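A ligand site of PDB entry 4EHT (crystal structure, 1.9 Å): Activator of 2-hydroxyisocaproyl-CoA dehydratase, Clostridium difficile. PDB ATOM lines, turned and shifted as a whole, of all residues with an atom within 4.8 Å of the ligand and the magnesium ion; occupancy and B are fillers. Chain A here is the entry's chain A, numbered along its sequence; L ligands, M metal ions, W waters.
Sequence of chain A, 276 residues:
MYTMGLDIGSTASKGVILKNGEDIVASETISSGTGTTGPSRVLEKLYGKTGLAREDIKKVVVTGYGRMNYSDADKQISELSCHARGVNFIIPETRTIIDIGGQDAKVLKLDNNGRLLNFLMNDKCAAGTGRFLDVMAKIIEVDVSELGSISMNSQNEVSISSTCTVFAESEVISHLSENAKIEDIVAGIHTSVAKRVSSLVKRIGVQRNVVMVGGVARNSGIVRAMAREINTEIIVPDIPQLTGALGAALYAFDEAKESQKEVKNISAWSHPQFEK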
ATOM      1  N   ASP A   7      13.891   7.669   4.054  1.00  0.00           N
ATOM      2  CA  ASP A   7      12.843   7.074   3.247  1.00  0.00           C
ATOM      3  C   ASP A   7      11.808   6.589   4.250  1.00  0.00           C
ATOM      4  O   ASP A   7      12.017   5.582   4.925  1.00  0.00           O
ATOM      5  CB  ASP A   7      13.416   5.913   2.417  1.00  0.00           C
ATOM      6  CG  ASP A   7      12.356   5.162   1.630  1.00  0.00           C
ATOM      7  OD1 ASP A   7      11.154   5.484   1.742  1.00  0.00           O
ATOM      8  OD2 ASP A   7      12.730   4.228   0.896  1.00  0.00           O
ATOM      9  N   GLY A   9       8.407   5.085   4.601  1.00  0.00           N
ATOM     10  CA  GLY A   9       7.292   4.371   3.992  1.00  0.00           C
ATOM     11  C   GLY A   9       6.161   4.153   4.995  1.00  0.00           C
ATOM     12  O   GLY A   9       6.232   4.584   6.144  1.00  0.00           O
ATOM     13  N   SER A  10       5.106   3.470   4.575  1.00  0.00           N
ATOM     14  CA  SER A  10       3.999   3.215   5.471  1.00  0.00           C
ATOM     15  C   SER A  10       4.282   2.013   6.373  1.00  0.00           C
ATOM     16  O   SER A  10       3.530   1.759   7.311  1.00  0.00           O
ATOM     17  CB  SER A  10       2.705   3.003   4.684  1.00  0.00           C
ATOM     18  OG  SER A  10       2.885   1.988   3.721  1.00  0.00           O
ATOM     19  N   THR A  11       5.363   1.281   6.096  1.00  0.00           N
ATOM     20  CA  THR A  11       5.712   0.116   6.909  1.00  0.00           C
ATOM     21  C   THR A  11       7.031   0.297   7.677  1.00  0.00           C
ATOM     22  O   THR A  11       7.129  -0.107   8.830  1.00  0.00           O
ATOM     23  CB  THR A  11       5.826  -1.159   6.037  1.00  0.00           C
ATOM     24  OG1 THR A  11       4.623  -1.346   5.294  1.00  0.00           O
ATOM     25  CG2 THR A  11       6.060  -2.393   6.907  1.00  0.00           C
ATOM     26  N   ALA A  12       8.033   0.887   7.025  1.00  0.00           N
ATOM     27  CA  ALA A  12       9.366   0.984   7.609  1.00  0.00           C
ATOM     28  C   ALA A  12      10.011   2.342   7.316  1.00  0.00           C
ATOM     29  O   ALA A  12       9.764   2.955   6.269  1.00  0.00           O
ATOM     30  CB  ALA A  12      10.231  -0.136   7.093  1.00  0.00           C
ATOM     31  N   LYS A  14      13.699   4.269   6.829  1.00  0.00           N
ATOM     32  CA  LYS A  14      15.063   3.910   6.443  1.00  0.00           C
ATOM     33  C   LYS A  14      15.881   5.166   6.310  1.00  0.00           C
ATOM     34  O   LYS A  14      15.418   6.152   5.745  1.00  0.00           O
ATOM     35  CB  LYS A  14      15.077   3.200   5.093  1.00  0.00           C
ATOM     36  CG  LYS A  14      14.558   1.755   5.084  1.00  0.00           C
ATOM     37  CD  LYS A  14      13.021   1.675   5.144  1.00  0.00           C
ATOM     38  CE  LYS A  14      12.368   2.124   3.846  1.00  0.00           C
ATOM     39  NZ  LYS A  14      10.914   1.783   3.858  1.00  0.00           N
ATOM     40  N   GLU A  79       9.692   8.999  -4.337  1.00  0.00           N
ATOM     41  CA  GLU A  79      10.392   7.742  -4.076  1.00  0.00           C
ATOM     42  C   GLU A  79      10.705   7.007  -5.372  1.00  0.00           C
ATOM     43  O   GLU A  79      11.622   6.200  -5.399  1.00  0.00           O
ATOM     44  CB  GLU A  79       9.611   6.849  -3.124  1.00  0.00           C
ATOM     45  CG  GLU A  79       8.293   6.289  -3.698  1.00  0.00           C
ATOM     46  CD  GLU A  79       7.431   5.661  -2.613  1.00  0.00           C
ATOM     47  OE1 GLU A  79       6.837   6.428  -1.806  1.00  0.00           O
ATOM     48  OE2 GLU A  79       7.346   4.413  -2.553  1.00  0.00           O
ATOM     49  N   HIS A  83      14.459   5.716  -5.645  1.00  0.00           N
ATOM     50  CA  HIS A  83      14.899   4.338  -5.824  1.00  0.00           C
ATOM     51  C   HIS A  83      15.726   4.188  -7.096  1.00  0.00           C
ATOM     52  O   HIS A  83      16.710   3.475  -7.118  1.00  0.00           O
ATOM     53  CB  HIS A  83      13.726   3.343  -5.808  1.00  0.00           C
ATOM     54  CG  HIS A  83      13.301   2.949  -4.434  1.00  0.00           C
ATOM     55  ND1 HIS A  83      14.031   2.082  -3.650  1.00  0.00           N
ATOM     56  CD2 HIS A  83      12.193   3.274  -3.709  1.00  0.00           C
ATOM     57  CE1 HIS A  83      13.421   1.914  -2.488  1.00  0.00           C
ATOM     58  NE2 HIS A  83      12.306   2.625  -2.507  1.00  0.00           N
ATOM     59  N   ASP A  99       9.968  -2.842  -6.960  1.00  0.00           N
ATOM     60  CA  ASP A  99      10.023  -2.419  -5.561  1.00  0.00           C
ATOM     61  C   ASP A  99       8.827  -3.071  -4.871  1.00  0.00           C
ATOM     62  O   ASP A  99       7.698  -2.645  -5.060  1.00  0.00           O
ATOM     63  CB  ASP A  99       9.960  -0.879  -5.524  1.00  0.00           C
ATOM     64  CG  ASP A  99       9.665  -0.298  -4.129  1.00  0.00           C
ATOM     65  OD1 ASP A  99       9.734  -1.019  -3.122  1.00  0.00           O
ATOM     66  OD2 ASP A  99       9.389   0.934  -4.047  1.00  0.00           O
ATOM     67  N   ILE A 100       9.063  -4.096  -4.071  1.00  0.00           N
ATOM     68  CA  ILE A 100       7.965  -4.720  -3.323  1.00  0.00           C
ATOM     69  C   ILE A 100       8.082  -4.285  -1.874  1.00  0.00           C
ATOM     70  O   ILE A 100       9.016  -4.692  -1.177  1.00  0.00           O
ATOM     71  CB  ILE A 100       8.003  -6.289  -3.406  1.00  0.00           C
ATOM     72  CG1 ILE A 100       8.082  -6.736  -4.862  1.00  0.00           C
ATOM     73  CG2 ILE A 100       6.752  -6.880  -2.742  1.00  0.00           C
ATOM     74  CD1 ILE A 100       8.024  -8.280  -5.047  1.00  0.00           C
ATOM     75  N   GLY A 101       7.145  -3.449  -1.420  1.00  0.00           N
ATOM     76  CA  GLY A 101       7.182  -2.963  -0.054  1.00  0.00           C
ATOM     77  C   GLY A 101       6.107  -3.564   0.819  1.00  0.00           C
ATOM     78  O   GLY A 101       5.536  -4.614   0.505  1.00  0.00           O
ATOM     79  N   GLY A 102       5.828  -2.907   1.938  1.00  0.00           N
ATOM     80  CA  GLY A 102       4.934  -3.448   2.944  1.00  0.00           C
ATOM     81  C   GLY A 102       3.484  -3.486   2.494  1.00  0.00           C
ATOM     82  O   GLY A 102       2.724  -4.334   2.951  1.00  0.00           O
ATOM     83  N   GLN A 103       3.094  -2.579   1.608  1.00  0.00           N
ATOM     84  CA  GLN A 103       1.687  -2.448   1.246  1.00  0.00           C
ATOM     85  C   GLN A 103       1.463  -2.210  -0.229  1.00  0.00           C
ATOM     86  O   GLN A 103       0.327  -1.983  -0.648  1.00  0.00           O
ATOM     87  CB  GLN A 103       1.035  -1.295   2.040  1.00  0.00           C
ATOM     88  CG  GLN A 103       1.042  -1.546   3.526  1.00  0.00           C
ATOM     89  CD  GLN A 103       0.258  -0.497   4.301  1.00  0.00           C
ATOM     90  OE1 GLN A 103      -0.511   0.277   3.740  1.00  0.00           O
ATOM     91  NE2 GLN A 103       0.464  -0.473   5.615  1.00  0.00           N
ATOM     92  N   LYS A 106       5.614  -1.997  -7.024  1.00  0.00           N
ATOM     93  CA  LYS A 106       5.798  -1.022  -8.100  1.00  0.00           C
ATOM     94  C   LYS A 106       6.763  -1.609  -9.125  1.00  0.00           C
ATOM     95  O   LYS A 106       7.733  -2.215  -8.723  1.00  0.00           O
ATOM     96  CB  LYS A 106       6.454   0.258  -7.546  1.00  0.00           C
ATOM     97  CG  LYS A 106       5.774   0.877  -6.344  1.00  0.00           C
ATOM     98  CD  LYS A 106       6.345   2.265  -6.023  1.00  0.00           C
ATOM     99  CE  LYS A 106       5.757   2.833  -4.745  1.00  0.00           C
ATOM    100  NZ  LYS A 106       6.220   2.065  -3.561  1.00  0.00           N
ATOM    101  N   GLY A 130       4.240  -7.168   0.778  1.00  0.00           N
ATOM    102  CA  GLY A 130       4.738  -7.624   2.065  1.00  0.00           C
ATOM    103  C   GLY A 130       3.656  -7.976   3.068  1.00  0.00           C
ATOM    104  O   GLY A 130       3.860  -8.830   3.930  1.00  0.00           O
ATOM    105  N   ARG A 131       2.499  -7.321   2.985  1.00  0.00           N
ATOM    106  CA  ARG A 131       1.413  -7.575   3.917  1.00  0.00           C
ATOM    107  C   ARG A 131       0.925  -9.014   3.793  1.00  0.00           C
ATOM    108  O   ARG A 131       0.641  -9.674   4.775  1.00  0.00           O
ATOM    109  CB  ARG A 131       0.247  -6.617   3.679  1.00  0.00           C
ATOM    110  CG  ARG A 131      -0.987  -6.932   4.534  1.00  0.00           C
ATOM    111  CD  ARG A 131      -0.709  -6.719   6.003  1.00  0.00           C
ATOM    112  NE  ARG A 131      -0.204  -5.381   6.218  1.00  0.00           N
ATOM    113  CZ  ARG A 131      -0.935  -4.340   6.583  1.00  0.00           C
ATOM    114  NH1 ARG A 131      -2.247  -4.475   6.801  1.00  0.00           N
ATOM    115  NH2 ARG A 131      -0.367  -3.150   6.739  1.00  0.00           N
ATOM    116  N   ASP A 134       3.425 -11.055   5.562  1.00  0.00           N
ATOM    117  CA  ASP A 134       3.346 -10.789   6.983  1.00  0.00           C
ATOM    118  C   ASP A 134       2.175 -11.552   7.598  1.00  0.00           C
ATOM    119  O   ASP A 134       2.330 -12.221   8.618  1.00  0.00           O
ATOM    120  CB  ASP A 134       3.280  -9.271   7.246  1.00  0.00           C
ATOM    121  CG  ASP A 134       4.526  -8.519   6.713  1.00  0.00           C
ATOM    122  OD1 ASP A 134       5.560  -9.164   6.400  1.00  0.00           O
ATOM    123  OD2 ASP A 134       4.455  -7.274   6.614  1.00  0.00           O
ATOM    124  N   VAL A 144       9.123 -13.553   9.182  1.00  0.00           N
ATOM    125  CA  VAL A 144       9.178 -13.292   7.747  1.00  0.00           C
ATOM    126  C   VAL A 144      10.620 -13.387   7.248  1.00  0.00           C
ATOM    127  O   VAL A 144      10.857 -13.710   6.079  1.00  0.00           O
ATOM    128  CB  VAL A 144       8.583 -11.893   7.368  1.00  0.00           C
ATOM    129  CG1 VAL A 144       7.110 -11.828   7.755  1.00  0.00           C
ATOM    130  CG2 VAL A 144       9.358 -10.768   7.996  1.00  0.00           C
ATOM    131  N   SER A 145      11.568 -13.139   8.142  1.00  0.00           N
ATOM    132  CA  SER A 145      12.992 -13.227   7.781  1.00  0.00           C
ATOM    133  C   SER A 145      13.466 -14.679   7.561  1.00  0.00           C
ATOM    134  O   SER A 145      14.543 -14.933   7.019  1.00  0.00           O
ATOM    135  CB  SER A 145      13.847 -12.534   8.850  1.00  0.00           C
ATOM    136  OG  SER A 145      13.856 -13.279  10.055  1.00  0.00           O
ATOM    137  N   GLY A 214      13.318  -2.967  -2.030  1.00  0.00           N
ATOM    138  CA  GLY A 214      12.228  -3.049  -1.073  1.00  0.00           C
ATOM    139  C   GLY A 214      12.555  -4.092  -0.027  1.00  0.00           C
ATOM    140  O   GLY A 214      13.424  -4.946  -0.253  1.00  0.00           O
ATOM    141  N   GLY A 215      11.902  -4.013   1.123  1.00  0.00           N
ATOM    142  CA  GLY A 215      12.190  -4.923   2.211  1.00  0.00           C
ATOM    143  C   GLY A 215      11.845  -6.362   1.869  1.00  0.00           C
ATOM    144  O   GLY A 215      12.429  -7.276   2.442  1.00  0.00           O
ATOM    145  N   VAL A 216      10.904  -6.565   0.953  1.00  0.00           N
ATOM    146  CA  VAL A 216      10.506  -7.928   0.567  1.00  0.00           C
ATOM    147  C   VAL A 216      11.574  -8.587  -0.314  1.00  0.00           C
ATOM    148  O   VAL A 216      11.670  -9.801  -0.346  1.00  0.00           O
ATOM    149  CB  VAL A 216       9.141  -7.969  -0.129  1.00  0.00           C
ATOM    150  CG1 VAL A 216       8.894  -9.348  -0.821  1.00  0.00           C
ATOM    151  CG2 VAL A 216       8.027  -7.667   0.872  1.00  0.00           C
ATOM    152  N   ARG A 218      14.486  -8.787   0.474  1.00  0.00           N
ATOM    153  CA  ARG A 218      15.387  -9.480   1.409  1.00  0.00           C
ATOM    154  C   ARG A 218      15.019 -10.962   1.548  1.00  0.00           C
ATOM    155  O   ARG A 218      15.764 -11.754   2.106  1.00  0.00           O
ATOM    156  CB  ARG A 218      15.330  -8.815   2.774  1.00  0.00           C
ATOM    157  CG  ARG A 218      15.836  -7.367   2.763  1.00  0.00           C
ATOM    158  CD  ARG A 218      15.672  -6.690   4.118  1.00  0.00           C
ATOM    159  NE  ARG A 218      16.614  -7.209   5.099  1.00  0.00           N
ATOM    160  CZ  ARG A 218      16.667  -6.801   6.367  1.00  0.00           C
ATOM    161  NH1 ARG A 218      15.822  -5.868   6.811  1.00  0.00           N
ATOM    162  NH2 ARG A 218      17.554  -7.327   7.197  1.00  0.00           N
ATOM    163  N   ASN A 219      13.829 -11.318   1.072  1.00  0.00           N
ATOM    164  CA  ASN A 219      13.370 -12.705   1.035  1.00  0.00           C
ATOM    165  C   ASN A 219      13.846 -13.390  -0.258  1.00  0.00           C
ATOM    166  O   ASN A 219      13.272 -13.178  -1.329  1.00  0.00           O
ATOM    167  CB  ASN A 219      11.830 -12.738   1.166  1.00  0.00           C
ATOM    168  CG  ASN A 219      11.257 -14.154   1.113  1.00  0.00           C
ATOM    169  OD1 ASN A 219      11.863 -15.070   0.562  1.00  0.00           O
ATOM    170  ND2 ASN A 219      10.075 -14.320   1.681  1.00  0.00           N
ATOM    171  N   GLN A 241      16.520  -2.877   0.896  1.00  0.00           N
ATOM    172  CA  GLN A 241      15.489  -2.072   1.548  1.00  0.00           C
ATOM    173  C   GLN A 241      15.895  -0.589   1.679  1.00  0.00           C
ATOM    174  O   GLN A 241      15.061   0.259   1.989  1.00  0.00           O
ATOM    175  CB  GLN A 241      15.151  -2.654   2.935  1.00  0.00           C
ATOM    176  CG  GLN A 241      13.848  -2.129   3.509  1.00  0.00           C
ATOM    177  CD  GLN A 241      13.493  -2.782   4.829  1.00  0.00           C
ATOM    178  OE1 GLN A 241      14.269  -3.548   5.376  1.00  0.00           O
ATOM    179  NE2 GLN A 241      12.312  -2.468   5.347  1.00  0.00           N
HETATM  180  P1  LIG L   1       7.778   0.594   2.762  1.00  0.00           P
HETATM  181  O1  LIG L   1       7.675   1.009   4.199  1.00  0.00           O
HETATM  182  O2  LIG L   1       6.495   0.640   1.970  1.00  0.00           O
HETATM  183  O3  LIG L   1       8.882   1.266   1.963  1.00  0.00           O
HETATM  184  P2  LIG L   1       9.670  -1.611   2.726  1.00  0.00           P
HETATM  185  O4  LIG L   1      10.440  -1.032   3.881  1.00  0.00           O
HETATM  186  O5  LIG L   1      10.232  -1.503   1.334  1.00  0.00           O
HETATM  187  O6  LIG L   1       8.163  -0.988   2.811  1.00  0.00           O
HETATM  188  O7  LIG L   1       9.426  -3.146   3.047  1.00  0.00           O
HETATM  189  C1  LIG L   1       8.661  -3.539   4.173  1.00  0.00           C
HETATM  190  C2  LIG L   1       8.428  -5.038   4.049  1.00  0.00           C
HETATM  191  O8  LIG L   1       9.657  -5.777   4.003  1.00  0.00           O
HETATM  192  C3  LIG L   1       7.655  -5.549   5.264  1.00  0.00           C
HETATM  193  O9  LIG L   1       6.443  -6.149   4.817  1.00  0.00           O
HETATM  194  C4  LIG L   1       8.602  -6.542   5.902  1.00  0.00           C
HETATM  195  O10 LIG L   1       7.987  -7.659   6.537  1.00  0.00           O
HETATM  196  C5  LIG L   1       9.508  -6.968   4.766  1.00  0.00           C
HETATM  197  N1  LIG L   1      10.798  -7.355   5.343  1.00  0.00           N
HETATM  198  C6  LIG L   1      11.511  -6.556   6.153  1.00  0.00           C
HETATM  199  N2  LIG L   1      12.660  -7.169   6.535  1.00  0.00           N
HETATM  200  C7  LIG L   1      12.685  -8.391   5.967  1.00  0.00           C
HETATM  201  C8  LIG L   1      13.618  -9.547   5.974  1.00  0.00           C
HETATM  202  N3  LIG L   1      14.766  -9.450   6.690  1.00  0.00           N
HETATM  203  N4  LIG L   1      13.290 -10.643   5.254  1.00  0.00           N
HETATM  204  C9  LIG L   1      12.129 -10.690   4.552  1.00  0.00           C
HETATM  205  N5  LIG L   1      11.223  -9.686   4.508  1.00  0.00           N
HETATM  206  C10 LIG L   1      11.443  -8.521   5.184  1.00  0.00           C
HETATM  207 MG    MG M   1       9.164   1.963  -0.049  1.00  0.00          MG
HETATM  208  O   HOH W   1       9.307   2.606  -2.152  1.00  0.00           O
HETATM  209  O   HOH W   2       9.471  -0.152  -0.628  1.00  0.00           O
HETATM  210  O   HOH W   3       5.270   2.902   1.705  1.00  0.00           O
HETATM  211  O   HOH W   4      16.926 -11.112   7.008  1.00  0.00           O
HETATM  212  O   HOH W   5       4.626  -0.506   0.357  1.00  0.00           O
HETATM  213  O   HOH W   6      14.967 -12.785   4.568  1.00  0.00           O
HETATM  214  O   HOH W   7      12.593  -0.160   0.863  1.00  0.00           O
HETATM  215  O   HOH W   8      11.342   2.211   0.258  1.00  0.00           O
HETATM  216  O   HOH W   9       8.660 -10.313   3.517  1.00  0.00           O
HETATM  217  O   HOH W  10       6.873   1.833  -0.193  1.00  0.00           O
HETATM  218  O   HOH W  11       9.132   4.092   0.546  1.00  0.00           O
HETATM  219  O   HOH W  12      14.851  -7.877   9.232  1.00  0.00           O
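Residues that only touch the magnesium ion: Glu 79 (3.9 Å). Of the 25 residues printed, 1 comes within 4 Å of the magnesium ion.
Water W1 lies within hydrogen-bond range of OD2 of Asp 99 (2.5 Å), OE2 of Glu 79 (2.7 Å), NE2 of His 83 (3.0 Å) and NZ of Lys 106 (3.4 Å). Water W2 lies within hydrogen-bond range of an oxygen (O5) of the ligand (2.5 Å) and the side-chain carboxylate (OD1) of Asp 99 (2.7 Å). Water W3 bridges an oxygen (O2) of the ligand (2.6 Å) and the backbone NH (N) of Ser 10 (2.9 Å). Water W5 lies within hydrogen-bond range of O2 of the ligand, N of Gln 103 and N of Gly 102. Water W7 bridges O of Gln 241 and O5 of the ligand. Water W12 lies within hydrogen-bond range of N3 of the ligand (3.0 Å) and NH1 of Arg 218 (3.3 Å).
The side-chain amide oxygen (OE1) of Gln 241 sits at hydrogen-bond distance from the guanidinium group (NH1) of Arg 218 (3.1 Å). The side-chain amino group of Lys 14 lies within hydrogen-bond range of the backbone carbonyl oxygen of Ala 12 (2.9 Å). O of Lys 14 is in hydrogen-bond range of N of Asp 7 (2.7 Å). The backbone carbonyl oxygen (O) of Gly 102 is in hydrogen-bond range of the backbone NH (N) of Arg 131 (3.0 Å). N of Val 216 sits at hydrogen-bond distance from O of Ile 100 (3.4 Å). The backbone NH (N) of Gly 130 lies within hydrogen-bond range of the backbone carbonyl oxygen (O) of Gly 101. NZ of Lys 106 lies within salt-bridge range of OE2 of Glu 79 (2.8 Å).
Gly 9 touches the ligand (CA to O1, 3.4 Å). Ser 10 touches the ligand (N to O1, 3.6 Å). Gly 101 touches the ligand. Gly 130 touches the ligand (CA to O9, 3.6 Å). O of Val 144 touches C9 of the ligand, at 3.6 Å. Ser 145 touches the ligand. CA of Gly 214 touches O5 of the ligand, 3.5 Å away. N of Asn 219 touches C9 of the ligand, 3.9 Å away. Of the 25 residues printed, 17 come within 4 Å of the ligand. The nearest printed residue that does not touch the ligand is Ile 100 (4.2 Å).
An oxygen (O4) of the ligand lies within hydrogen-bond range of the side-chain amide nitrogen (NE2) of Gln 241, at 2.8 Å. The side-chain amino group of Lys 14 lies within salt-bridge range of an oxygen (O4) of the ligand (2.9 Å). An oxygen (O1) of the ligand lies within hydrogen-bond range of the backbone NH (N) of Ala 12, 2.9 Å away. An oxygen (O10) of the ligand lies within hydrogen-bond range of the side-chain carboxylate (OD1) of Asp 134 (2.9 Å). The backbone NH of Thr 11 is in hydrogen-bond range of an oxygen (O1) of the ligand (3.0 Å). The backbone NH (N) of Gly 215 lies within hydrogen-bond range of an oxygen (O5) of the ligand (3.0 Å). An oxygen (O6) of the ligand is in hydrogen-bond range of the backbone NH (N) of Gly 102, at 3.1 Å. The guanidinium group (NH1) of Arg 218 is in hydrogen-bond range of a nitrogen (N2) of the ligand (3.4 Å). An oxygen (O8) of the ligand sits at hydrogen-bond distance from the backbone NH (N) of Val 216, at 3.4 Å.
The magnesium ion is bound by an oxygen (O3) of the ligand (2.1 Å), water W1 (2.2 Å), water W11 (2.2 Å), water W8 (2.2 Å), water W2 (2.2 Å) and water W10 (2.3 Å). The magnesium ion has six donor atoms within binding distance.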
